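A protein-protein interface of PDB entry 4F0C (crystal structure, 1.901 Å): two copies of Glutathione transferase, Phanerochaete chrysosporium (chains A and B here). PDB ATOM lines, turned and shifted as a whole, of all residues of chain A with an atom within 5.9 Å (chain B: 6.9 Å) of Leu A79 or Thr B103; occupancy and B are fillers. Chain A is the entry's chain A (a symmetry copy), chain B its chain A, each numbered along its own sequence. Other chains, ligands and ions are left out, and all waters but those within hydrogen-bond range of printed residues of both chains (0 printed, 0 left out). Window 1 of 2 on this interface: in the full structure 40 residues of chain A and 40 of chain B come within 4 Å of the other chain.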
ATOM      1  N   LEU A  24       7.334  -5.222 -13.759  1.00  0.00           N
ATOM      2  CA  LEU A  24       7.480  -5.533 -15.187  1.00  0.00           C
ATOM      3  C   LEU A  24       6.468  -4.795 -16.051  1.00  0.00           C
ATOM      4  O   LEU A  24       6.808  -4.289 -17.122  1.00  0.00           O
ATOM      5  CB  LEU A  24       7.419  -7.056 -15.451  1.00  0.00           C
ATOM      6  CG  LEU A  24       7.437  -7.434 -16.953  1.00  0.00           C
ATOM      7  CD1 LEU A  24       8.784  -7.000 -17.561  1.00  0.00           C
ATOM      8  CD2 LEU A  24       7.285  -8.947 -17.070  1.00  0.00           C
ATOM      9  N   SER A  74       3.626 -15.831  -9.740  1.00  0.00           N
ATOM     10  CA  SER A  74       4.301 -14.590 -10.132  1.00  0.00           C
ATOM     11  C   SER A  74       5.356 -14.779 -11.238  1.00  0.00           C
ATOM     12  O   SER A  74       5.385 -14.001 -12.193  1.00  0.00           O
ATOM     13  CB  SER A  74       4.919 -13.871  -8.903  1.00  0.00           C
ATOM     14  OG  SER A  74       5.906 -14.659  -8.219  1.00  0.00           O
ATOM     15  N   ASP A  75       6.213 -15.806 -11.135  1.00  0.00           N
ATOM     16  CA  ASP A  75       7.294 -15.894 -12.117  1.00  0.00           C
ATOM     17  C   ASP A  75       6.802 -16.434 -13.462  1.00  0.00           C
ATOM     18  O   ASP A  75       7.386 -16.126 -14.521  1.00  0.00           O
ATOM     19  CB  ASP A  75       8.483 -16.753 -11.612  1.00  0.00           C
ATOM     20  CG  ASP A  75       9.298 -16.051 -10.541  1.00  0.00           C
ATOM     21  OD1 ASP A  75       9.003 -14.867 -10.183  1.00  0.00           O
ATOM     22  OD2 ASP A  75      10.269 -16.672 -10.078  1.00  0.00           O
ATOM     23  N   ALA A  76       5.757 -17.261 -13.436  1.00  0.00           N
ATOM     24  CA  ALA A  76       5.146 -17.659 -14.717  1.00  0.00           C
ATOM     25  C   ALA A  76       4.462 -16.477 -15.396  1.00  0.00           C
ATOM     26  O   ALA A  76       4.482 -16.360 -16.625  1.00  0.00           O
ATOM     27  CB  ALA A  76       4.159 -18.802 -14.524  1.00  0.00           C
ATOM     28  N   ILE A  77       3.833 -15.615 -14.602  1.00  0.00           N
ATOM     29  CA  ILE A  77       3.274 -14.367 -15.126  1.00  0.00           C
ATOM     30  C   ILE A  77       4.350 -13.502 -15.809  1.00  0.00           C
ATOM     31  O   ILE A  77       4.113 -12.952 -16.911  1.00  0.00           O
ATOM     32  CB  ILE A  77       2.566 -13.562 -14.003  1.00  0.00           C
ATOM     33  CG1 ILE A  77       1.360 -14.360 -13.485  1.00  0.00           C
ATOM     34  CG2 ILE A  77       2.095 -12.164 -14.506  1.00  0.00           C
ATOM     35  CD1 ILE A  77       0.763 -13.774 -12.212  1.00  0.00           C
ATOM     36  N   LEU A  78       5.524 -13.401 -15.179  1.00  0.00           N
ATOM     37  CA  LEU A  78       6.623 -12.639 -15.790  1.00  0.00           C
ATOM     38  C   LEU A  78       6.990 -13.223 -17.157  1.00  0.00           C
ATOM     39  O   LEU A  78       7.164 -12.470 -18.110  1.00  0.00           O
ATOM     40  CB  LEU A  78       7.875 -12.593 -14.897  1.00  0.00           C
ATOM     41  CG  LEU A  78       7.730 -11.966 -13.497  1.00  0.00           C
ATOM     42  CD1 LEU A  78       9.030 -12.132 -12.661  1.00  0.00           C
ATOM     43  CD2 LEU A  78       7.328 -10.468 -13.584  1.00  0.00           C
ATOM     44  N   LEU A  79       7.096 -14.546 -17.239  1.00  0.00           N
ATOM     45  CA  LEU A  79       7.402 -15.214 -18.501  1.00  0.00           C
ATOM     46  C   LEU A  79       6.324 -14.970 -19.537  1.00  0.00           C
ATOM     47  O   LEU A  79       6.634 -14.738 -20.702  1.00  0.00           O
ATOM     48  CB  LEU A  79       7.628 -16.730 -18.266  1.00  0.00           C
ATOM     49  CG  LEU A  79       9.002 -16.978 -17.621  1.00  0.00           C
ATOM     50  CD1 LEU A  79       9.030 -18.348 -16.915  1.00  0.00           C
ATOM     51  CD2 LEU A  79      10.141 -16.899 -18.698  1.00  0.00           C
ATOM     52  N   TYR A  80       5.061 -15.058 -19.121  1.00  0.00           N
ATOM     53  CA  TYR A  80       3.928 -14.843 -20.025  1.00  0.00           C
ATOM     54  C   TYR A  80       4.043 -13.442 -20.638  1.00  0.00           C
ATOM     55  O   TYR A  80       3.961 -13.269 -21.855  1.00  0.00           O
ATOM     56  CB  TYR A  80       2.587 -14.954 -19.275  1.00  0.00           C
ATOM     57  CG  TYR A  80       1.357 -14.555 -20.119  1.00  0.00           C
ATOM     58  CD1 TYR A  80       0.762 -15.459 -21.000  1.00  0.00           C
ATOM     59  CD2 TYR A  80       0.821 -13.267 -20.024  1.00  0.00           C
ATOM     60  CE1 TYR A  80      -0.358 -15.092 -21.790  1.00  0.00           C
ATOM     61  CE2 TYR A  80      -0.288 -12.874 -20.821  1.00  0.00           C
ATOM     62  CZ  TYR A  80      -0.867 -13.790 -21.681  1.00  0.00           C
ATOM     63  OH  TYR A  80      -1.961 -13.418 -22.436  1.00  0.00           O
ATOM     64  N   ILE A  81       4.255 -12.455 -19.781  1.00  0.00           N
ATOM     65  CA  ILE A  81       4.301 -11.079 -20.252  1.00  0.00           C
ATOM     66  C   ILE A  81       5.447 -10.850 -21.245  1.00  0.00           C
ATOM     67  O   ILE A  81       5.255 -10.211 -22.303  1.00  0.00           O
ATOM     68  CB  ILE A  81       4.401 -10.097 -19.083  1.00  0.00           C
ATOM     69  CG1 ILE A  81       3.098 -10.132 -18.274  1.00  0.00           C
ATOM     70  CG2 ILE A  81       4.635  -8.646 -19.618  1.00  0.00           C
ATOM     71  CD1 ILE A  81       3.184  -9.421 -16.933  1.00  0.00           C
ATOM     72  N   VAL A  82       6.646 -11.349 -20.935  1.00  0.00           N
ATOM     73  CA  VAL A  82       7.747 -11.119 -21.886  1.00  0.00           C
ATOM     74  C   VAL A  82       7.625 -11.945 -23.169  1.00  0.00           C
ATOM     75  O   VAL A  82       8.034 -11.475 -24.243  1.00  0.00           O
ATOM     76  CB  VAL A  82       9.181 -11.261 -21.287  1.00  0.00           C
ATOM     77  CG1 VAL A  82       9.398 -10.217 -20.175  1.00  0.00           C
ATOM     78  CG2 VAL A  82       9.462 -12.697 -20.794  1.00  0.00           C
ATOM     79  N   GLU A  83       7.099 -13.164 -23.085  1.00  0.00           N
ATOM     80  CA  GLU A  83       6.904 -13.924 -24.313  1.00  0.00           C
ATOM     81  C   GLU A  83       5.966 -13.192 -25.281  1.00  0.00           C
ATOM     82  O   GLU A  83       6.223 -13.099 -26.495  1.00  0.00           O
ATOM     83  CB  GLU A  83       6.402 -15.339 -23.996  1.00  0.00           C
ATOM     84  CG  GLU A  83       7.532 -16.249 -23.518  1.00  0.00           C
ATOM     85  CD  GLU A  83       8.456 -16.674 -24.662  1.00  0.00           C
ATOM     86  OE1 GLU A  83       9.604 -17.080 -24.392  1.00  0.00           O
ATOM     87  OE2 GLU A  83       8.026 -16.611 -25.833  1.00  0.00           O
ATOM     88  N   LYS A  84       4.885 -12.641 -24.748  1.00  0.00           N
ATOM     89  CA  LYS A  84       3.872 -12.076 -25.630  1.00  0.00           C
ATOM     90  C   LYS A  84       4.006 -10.586 -25.903  1.00  0.00           C
ATOM     91  O   LYS A  84       3.513 -10.108 -26.917  1.00  0.00           O
ATOM     92  CB  LYS A  84       2.453 -12.387 -25.099  1.00  0.00           C
ATOM     93  CG  LYS A  84       2.012 -13.814 -25.415  1.00  0.00           C
ATOM     94  CD  LYS A  84       0.510 -14.073 -25.157  1.00  0.00           C
ATOM     95  CE  LYS A  84      -0.441 -13.149 -25.902  1.00  0.00           C
ATOM     96  NZ  LYS A  84      -0.598 -13.407 -27.371  1.00  0.00           N
ATOM     97  N   MET A 102      17.801 -18.085 -18.304  1.00  0.00           N
ATOM     98  CA  MET A 102      16.922 -17.106 -17.643  1.00  0.00           C
ATOM     99  C   MET A 102      15.858 -17.843 -16.807  1.00  0.00           C
ATOM    100  O   MET A 102      15.522 -17.445 -15.678  1.00  0.00           O
ATOM    101  CB  MET A 102      16.287 -16.172 -18.676  1.00  0.00           C
ATOM    102  CG  MET A 102      15.516 -14.989 -18.058  1.00  0.00           C
ATOM    103  SD  MET A 102      14.756 -13.925 -19.300  1.00  0.00           S
ATOM    104  CE  MET A 102      13.390 -14.961 -19.847  1.00  0.00           C
ATOM    105  N   THR A 103      15.333 -18.927 -17.368  1.00  0.00           N
ATOM    106  CA  THR A 103      14.348 -19.757 -16.665  1.00  0.00           C
ATOM    107  C   THR A 103      14.928 -20.429 -15.413  1.00  0.00           C
ATOM    108  O   THR A 103      14.276 -20.496 -14.365  1.00  0.00           O
ATOM    109  CB  THR A 103      13.712 -20.768 -17.631  1.00  0.00           C
ATOM    110  OG1 THR A 103      12.950 -20.033 -18.575  1.00  0.00           O
ATOM    111  CG2 THR A 103      12.765 -21.743 -16.924  1.00  0.00           C
ATOM    112  N   LEU A 106      15.029 -17.875 -12.753  1.00  0.00           N
ATOM    113  CA  LEU A 106      13.657 -17.674 -12.249  1.00  0.00           C
ATOM    114  C   LEU A 106      13.239 -18.798 -11.288  1.00  0.00           C
ATOM    115  O   LEU A 106      12.623 -18.546 -10.239  1.00  0.00           O
ATOM    116  CB  LEU A 106      12.632 -17.550 -13.396  1.00  0.00           C
ATOM    117  CG  LEU A 106      12.778 -16.256 -14.200  1.00  0.00           C
ATOM    118  CD1 LEU A 106      12.019 -16.349 -15.556  1.00  0.00           C
ATOM    119  CD2 LEU A 106      12.230 -15.103 -13.355  1.00  0.00           C
ATOM    120  N   PHE A 107      13.566 -20.034 -11.642  1.00  0.00           N
ATOM    121  CA  PHE A 107      13.266 -21.150 -10.741  1.00  0.00           C
ATOM    122  C   PHE A 107      14.035 -21.026  -9.444  1.00  0.00           C
ATOM    123  O   PHE A 107      13.512 -21.381  -8.374  1.00  0.00           O
ATOM    124  CB  PHE A 107      13.498 -22.524 -11.396  1.00  0.00           C
ATOM    125  CG  PHE A 107      12.269 -23.021 -12.152  1.00  0.00           C
ATOM    126  CD1 PHE A 107      11.197 -23.618 -11.459  1.00  0.00           C
ATOM    127  CD2 PHE A 107      12.153 -22.829 -13.522  1.00  0.00           C
ATOM    128  CE1 PHE A 107      10.039 -24.039 -12.150  1.00  0.00           C
ATOM    129  CE2 PHE A 107      11.011 -23.251 -14.224  1.00  0.00           C
ATOM    130  CZ  PHE A 107       9.950 -23.841 -13.547  1.00  0.00           C
ATOM    131  N   ILE A 168      13.925 -10.250 -16.766  1.00  0.00           N
ATOM    132  CA  ILE A 168      13.026 -10.593 -15.678  1.00  0.00           C
ATOM    133  C   ILE A 168      13.708 -11.504 -14.646  1.00  0.00           C
ATOM    134  O   ILE A 168      13.239 -11.572 -13.514  1.00  0.00           O
ATOM    135  CB  ILE A 168      11.703 -11.225 -16.183  1.00  0.00           C
ATOM    136  CG1 ILE A 168      11.987 -12.364 -17.199  1.00  0.00           C
ATOM    137  CG2 ILE A 168      10.843 -10.119 -16.827  1.00  0.00           C
ATOM    138  CD1 ILE A 168      10.754 -13.317 -17.401  1.00  0.00           C
ATOM    139  N   LEU B  79      12.558 -28.781 -18.132  1.00  0.00           N
ATOM    140  CA  LEU B  79      12.243 -27.964 -19.301  1.00  0.00           C
ATOM    141  C   LEU B  79      13.312 -28.080 -20.367  1.00  0.00           C
ATOM    142  O   LEU B  79      12.991 -28.169 -21.550  1.00  0.00           O
ATOM    143  CB  LEU B  79      12.018 -26.489 -18.881  1.00  0.00           C
ATOM    144  CG  LEU B  79      10.650 -26.321 -18.199  1.00  0.00           C
ATOM    145  CD1 LEU B  79      10.629 -25.048 -17.331  1.00  0.00           C
ATOM    146  CD2 LEU B  79       9.503 -26.270 -19.268  1.00  0.00           C
ATOM    147  N   VAL B  93       4.447 -30.059 -24.450  1.00  0.00           N
ATOM    148  CA  VAL B  93       3.393 -29.479 -25.287  1.00  0.00           C
ATOM    149  C   VAL B  93       3.958 -28.574 -26.372  1.00  0.00           C
ATOM    150  O   VAL B  93       5.094 -28.103 -26.262  1.00  0.00           O
ATOM    151  CB  VAL B  93       2.349 -28.693 -24.424  1.00  0.00           C
ATOM    152  CG1 VAL B  93       1.528 -29.664 -23.573  1.00  0.00           C
ATOM    153  CG2 VAL B  93       3.013 -27.653 -23.516  1.00  0.00           C
ATOM    154  N   PHE B  96       1.895 -22.192 -27.584  1.00  0.00           N
ATOM    155  CA  PHE B  96       2.241 -21.218 -26.546  1.00  0.00           C
ATOM    156  C   PHE B  96       1.321 -21.317 -25.329  1.00  0.00           C
ATOM    157  O   PHE B  96       1.801 -21.386 -24.180  1.00  0.00           O
ATOM    158  CB  PHE B  96       2.214 -19.775 -27.061  1.00  0.00           C
ATOM    159  CG  PHE B  96       2.341 -18.786 -25.955  1.00  0.00           C
ATOM    160  CD1 PHE B  96       3.557 -18.614 -25.310  1.00  0.00           C
ATOM    161  CD2 PHE B  96       1.231 -18.117 -25.475  1.00  0.00           C
ATOM    162  CE1 PHE B  96       3.687 -17.730 -24.239  1.00  0.00           C
ATOM    163  CE2 PHE B  96       1.356 -17.230 -24.413  1.00  0.00           C
ATOM    164  CZ  PHE B  96       2.595 -17.040 -23.797  1.00  0.00           C
ATOM    165  N   ASP B  98      -0.433 -23.737 -24.158  1.00  0.00           N
ATOM    166  CA  ASP B  98      -0.180 -24.915 -23.339  1.00  0.00           C
ATOM    167  C   ASP B  98       1.176 -24.809 -22.618  1.00  0.00           C
ATOM    168  O   ASP B  98       1.300 -25.176 -21.439  1.00  0.00           O
ATOM    169  CB  ASP B  98      -0.206 -26.204 -24.182  1.00  0.00           C
ATOM    170  CG  ASP B  98      -1.608 -26.595 -24.640  1.00  0.00           C
ATOM    171  OD1 ASP B  98      -2.596 -26.110 -24.059  1.00  0.00           O
ATOM    172  OD2 ASP B  98      -1.710 -27.442 -25.555  1.00  0.00           O
ATOM    173  N   LYS B  99       2.201 -24.338 -23.325  1.00  0.00           N
ATOM    174  CA  LYS B  99       3.522 -24.208 -22.712  1.00  0.00           C
ATOM    175  C   LYS B  99       3.525 -23.308 -21.477  1.00  0.00           C
ATOM    176  O   LYS B  99       4.174 -23.623 -20.471  1.00  0.00           O
ATOM    177  CB  LYS B  99       4.546 -23.664 -23.712  1.00  0.00           C
ATOM    178  CG  LYS B  99       5.016 -24.682 -24.751  1.00  0.00           C
ATOM    179  CD  LYS B  99       5.975 -23.995 -25.745  1.00  0.00           C
ATOM    180  CE  LYS B  99       6.392 -24.920 -26.867  1.00  0.00           C
ATOM    181  NZ  LYS B  99       7.375 -24.172 -27.746  1.00  0.00           N
ATOM    182  N   ILE B 100       2.848 -22.177 -21.555  1.00  0.00           N
ATOM    183  CA  ILE B 100       2.900 -21.258 -20.422  1.00  0.00           C
ATOM    184  C   ILE B 100       2.155 -21.839 -19.216  1.00  0.00           C
ATOM    185  O   ILE B 100       2.557 -21.635 -18.051  1.00  0.00           O
ATOM    186  CB  ILE B 100       2.422 -19.850 -20.768  1.00  0.00           C
ATOM    187  CG1 ILE B 100       2.766 -18.869 -19.628  1.00  0.00           C
ATOM    188  CG2 ILE B 100       0.902 -19.826 -21.178  1.00  0.00           C
ATOM    189  CD1 ILE B 100       4.284 -18.730 -19.369  1.00  0.00           C
ATOM    190  N   ILE B 101       1.093 -22.596 -19.480  1.00  0.00           N
ATOM    191  CA  ILE B 101       0.364 -23.207 -18.364  1.00  0.00           C
ATOM    192  C   ILE B 101       1.165 -24.397 -17.802  1.00  0.00           C
ATOM    193  O   ILE B 101       1.198 -24.620 -16.589  1.00  0.00           O
ATOM    194  CB  ILE B 101      -1.064 -23.637 -18.818  1.00  0.00           C
ATOM    195  CG1 ILE B 101      -1.865 -22.398 -19.232  1.00  0.00           C
ATOM    196  CG2 ILE B 101      -1.780 -24.459 -17.700  1.00  0.00           C
ATOM    197  CD1 ILE B 101      -1.934 -21.282 -18.119  1.00  0.00           C
ATOM    198  N   MET B 102       1.847 -25.144 -18.669  1.00  0.00           N
ATOM    199  CA  MET B 102       2.730 -26.197 -18.139  1.00  0.00           C
ATOM    200  C   MET B 102       3.802 -25.566 -17.228  1.00  0.00           C
ATOM    201  O   MET B 102       4.147 -26.098 -16.160  1.00  0.00           O
ATOM    202  CB  MET B 102       3.357 -26.997 -19.284  1.00  0.00           C
ATOM    203  CG  MET B 102       4.132 -28.247 -18.821  1.00  0.00           C
ATOM    204  SD  MET B 102       4.882 -29.150 -20.190  1.00  0.00           S
ATOM    205  CE  MET B 102       6.243 -28.055 -20.617  1.00  0.00           C
ATOM    206  N   THR B 103       4.322 -24.422 -17.658  1.00  0.00           N
ATOM    207  CA  THR B 103       5.314 -23.683 -16.867  1.00  0.00           C
ATOM    208  C   THR B 103       4.744 -23.168 -15.538  1.00  0.00           C
ATOM    209  O   THR B 103       5.405 -23.229 -14.494  1.00  0.00           O
ATOM    210  CB  THR B 103       5.942 -22.561 -17.709  1.00  0.00           C
ATOM    211  OG1 THR B 103       6.696 -23.176 -18.741  1.00  0.00           O
ATOM    212  CG2 THR B 103       6.895 -21.679 -16.896  1.00  0.00           C
ATOM    213  N   GLN B 104       3.524 -22.654 -15.584  1.00  0.00           N
ATOM    214  CA  GLN B 104       2.832 -22.237 -14.366  1.00  0.00           C
ATOM    215  C   GLN B 104       2.767 -23.384 -13.338  1.00  0.00           C
ATOM    216  O   GLN B 104       3.088 -23.197 -12.178  1.00  0.00           O
ATOM    217  CB  GLN B 104       1.414 -21.821 -14.732  1.00  0.00           C
ATOM    218  CG  GLN B 104       0.466 -21.527 -13.539  1.00  0.00           C
ATOM    219  CD  GLN B 104      -0.967 -21.491 -14.009  1.00  0.00           C
ATOM    220  OE1 GLN B 104      -1.482 -20.430 -14.377  1.00  0.00           O
ATOM    221  NE2 GLN B 104      -1.622 -22.692 -14.055  1.00  0.00           N
ATOM    222  N   TRP B 105       2.330 -24.571 -13.774  1.00  0.00           N
ATOM    223  CA  TRP B 105       2.259 -25.709 -12.869  1.00  0.00           C
ATOM    224  C   TRP B 105       3.642 -26.116 -12.359  1.00  0.00           C
ATOM    225  O   TRP B 105       3.770 -26.515 -11.205  1.00  0.00           O
ATOM    226  CB  TRP B 105       1.518 -26.886 -13.517  1.00  0.00           C
ATOM    227  CG  TRP B 105       0.015 -26.628 -13.474  1.00  0.00           C
ATOM    228  CD1 TRP B 105      -0.767 -26.165 -14.492  1.00  0.00           C
ATOM    229  CD2 TRP B 105      -0.831 -26.764 -12.331  1.00  0.00           C
ATOM    230  NE1 TRP B 105      -2.076 -26.029 -14.059  1.00  0.00           N
ATOM    231  CE2 TRP B 105      -2.134 -26.387 -12.729  1.00  0.00           C
ATOM    232  CE3 TRP B 105      -0.613 -27.200 -11.007  1.00  0.00           C
ATOM    233  CZ2 TRP B 105      -3.234 -26.426 -11.850  1.00  0.00           C
ATOM    234  CZ3 TRP B 105      -1.713 -27.227 -10.113  1.00  0.00           C
ATOM    235  CH2 TRP B 105      -2.995 -26.820 -10.544  1.00  0.00           C
ATOM    236  N   LEU B 106       4.664 -26.027 -13.208  1.00  0.00           N
ATOM    237  CA  LEU B 106       6.041 -26.287 -12.744  1.00  0.00           C
ATOM    238  C   LEU B 106       6.467 -25.288 -11.657  1.00  0.00           C
ATOM    239  O   LEU B 106       7.092 -25.667 -10.651  1.00  0.00           O
ATOM    240  CB  LEU B 106       7.056 -26.271 -13.905  1.00  0.00           C
ATOM    241  CG  LEU B 106       6.903 -27.457 -14.859  1.00  0.00           C
ATOM    242  CD1 LEU B 106       7.650 -27.199 -16.200  1.00  0.00           C
ATOM    243  CD2 LEU B 106       7.457 -28.704 -14.166  1.00  0.00           C
ATOM    244  N   PHE B 107       6.138 -24.019 -11.854  1.00  0.00           N
ATOM    245  CA  PHE B 107       6.445 -23.021 -10.827  1.00  0.00           C
ATOM    246  C   PHE B 107       5.688 -23.303  -9.548  1.00  0.00           C
ATOM    247  O   PHE B 107       6.220 -23.080  -8.447  1.00  0.00           O
ATOM    248  CB  PHE B 107       6.209 -21.578 -11.308  1.00  0.00           C
ATOM    249  CG  PHE B 107       7.432 -20.992 -12.007  1.00  0.00           C
ATOM    250  CD1 PHE B 107       8.509 -20.483 -11.256  1.00  0.00           C
ATOM    251  CD2 PHE B 107       7.536 -21.015 -13.392  1.00  0.00           C
ATOM    252  CE1 PHE B 107       9.662 -19.980 -11.901  1.00  0.00           C
ATOM    253  CE2 PHE B 107       8.672 -20.510 -14.047  1.00  0.00           C
ATOM    254  CZ  PHE B 107       9.740 -20.007 -13.312  1.00  0.00           C
ATOM    255  N   PHE B 108       4.459 -23.791  -9.679  1.00  0.00           N
ATOM    256  CA  PHE B 108       3.706 -24.164  -8.469  1.00  0.00           C
ATOM    257  C   PHE B 108       4.399 -25.331  -7.747  1.00  0.00           C
ATOM    258  O   PHE B 108       4.557 -25.324  -6.521  1.00  0.00           O
ATOM    259  CB  PHE B 108       2.229 -24.474  -8.775  1.00  0.00           C
ATOM    260  CG  PHE B 108       1.457 -24.982  -7.561  1.00  0.00           C
ATOM    261  CD1 PHE B 108       1.499 -24.294  -6.366  1.00  0.00           C
ATOM    262  CD2 PHE B 108       0.719 -26.154  -7.624  1.00  0.00           C
ATOM    263  CE1 PHE B 108       0.787 -24.759  -5.207  1.00  0.00           C
ATOM    264  CE2 PHE B 108      -0.001 -26.624  -6.492  1.00  0.00           C
ATOM    265  CZ  PHE B 108       0.043 -25.917  -5.282  1.00  0.00           C
ATOM    266  N   GLN B 109       4.835 -26.318  -8.514  1.00  0.00           N
ATOM    267  CA  GLN B 109       5.580 -27.427  -7.909  1.00  0.00           C
ATOM    268  C   GLN B 109       6.836 -26.866  -7.209  1.00  0.00           C
ATOM    269  O   GLN B 109       7.139 -27.205  -6.053  1.00  0.00           O
ATOM    270  CB  GLN B 109       6.019 -28.441  -8.981  1.00  0.00           C
ATOM    271  CG  GLN B 109       6.600 -29.735  -8.373  1.00  0.00           C
ATOM    272  CD  GLN B 109       8.035 -29.539  -7.847  1.00  0.00           C
ATOM    273  OE1 GLN B 109       8.878 -28.935  -8.521  1.00  0.00           O
ATOM    274  NE2 GLN B 109       8.316 -30.058  -6.633  1.00  0.00           N
ATOM    275  N   VAL B 162      -2.134 -30.418 -17.536  1.00  0.00           N
ATOM    276  CA  VAL B 162      -2.188 -29.527 -18.704  1.00  0.00           C
ATOM    277  C   VAL B 162      -2.501 -30.275 -19.954  1.00  0.00           C
ATOM    278  O   VAL B 162      -1.973 -31.364 -20.169  1.00  0.00           O
ATOM    279  CB  VAL B 162      -0.825 -28.805 -18.933  1.00  0.00           C
ATOM    280  CG1 VAL B 162      -0.968 -27.758 -20.045  1.00  0.00           C
ATOM    281  CG2 VAL B 162      -0.360 -28.134 -17.593  1.00  0.00           C
ATOM    282  N   ALA B 169       4.867 -31.406 -16.150  1.00  0.00           N
ATOM    283  CA  ALA B 169       4.161 -30.757 -15.026  1.00  0.00           C
ATOM    284  C   ALA B 169       3.715 -31.829 -14.039  1.00  0.00           C
ATOM    285  O   ALA B 169       3.954 -31.692 -12.847  1.00  0.00           O
ATOM    286  CB  ALA B 169       2.974 -29.908 -15.469  1.00  0.00           C
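Among the printed residues, 14 pairs touch across the chains.
The side-chain hydroxyl (OG1) of Thr B103 lies within hydrogen-bond range of the backbone carbonyl oxygen (O) of Lys B99, 3.1 Å away. The side-chain amide nitrogen (NE2) of Gln B104 sits close to the indole nitrogen (NE1) of Trp B105 (3.4 Å).
Among the printed residues, pairs that only touch across the chains: Asp A75 with Phe B107 (3.4 Å), Ala A76 with Ile B100 (3.6 Å), Ala A76 with Gln B104 (3.7 Å), Leu A79 with Thr B103 (3.96 Å), Leu A79 with Phe B107 (3.6 Å), Tyr A80 with Phe B96 (3.7 Å), Tyr A80 with Ile B100 (3.8 Å), Glu A83 with Phe B96 (3.6 Å), Lys A84 with Phe B96 (3.4 Å), Thr A103 with Leu B79 (3.96 Å), Leu A106 with Phe B107 (3.7 Å), Phe A107 with Leu B79 (3.6 Å), Phe A107 with Leu B106 (3.7 Å) and Phe A107 with Phe B107 (3.6 Å).
Leu A79 touches Thr B103, and with the chains exchanged Thr A103 touches Leu B79. Leu A79 touches Phe B107, and with the chains exchanged Phe A107 touches Leu B79. Leu A106 touches Phe B107, and with the chains exchanged Phe A107 touches Leu B106. Phe A107 touches its own counterpart, Phe B107.
Printed residues of chain B within 4 Å of Ala A76: Ile B100 and Gln B104. Printed residues of chain B within 4 Å of Glu A83: Phe B96. Ile A168 touches none of the printed residues of chain B. Of the printed residues of chain A, Leu B79 touches Thr A103 and Phe A107. Of the printed residues of chain A, Phe B96 touches Tyr A80 (3.7 Å), Glu A83 (3.6 Å) and Lys A84 (3.4 Å). Printed residues of chain A within 4 Å of Thr B103: Leu A79. The nearest residue of chain B that does not touch Leu A79 is Ile B100 (4.05 Å). The nearest residue of chain A that does not touch Thr B103 is Ala A76 (4.5 Å).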
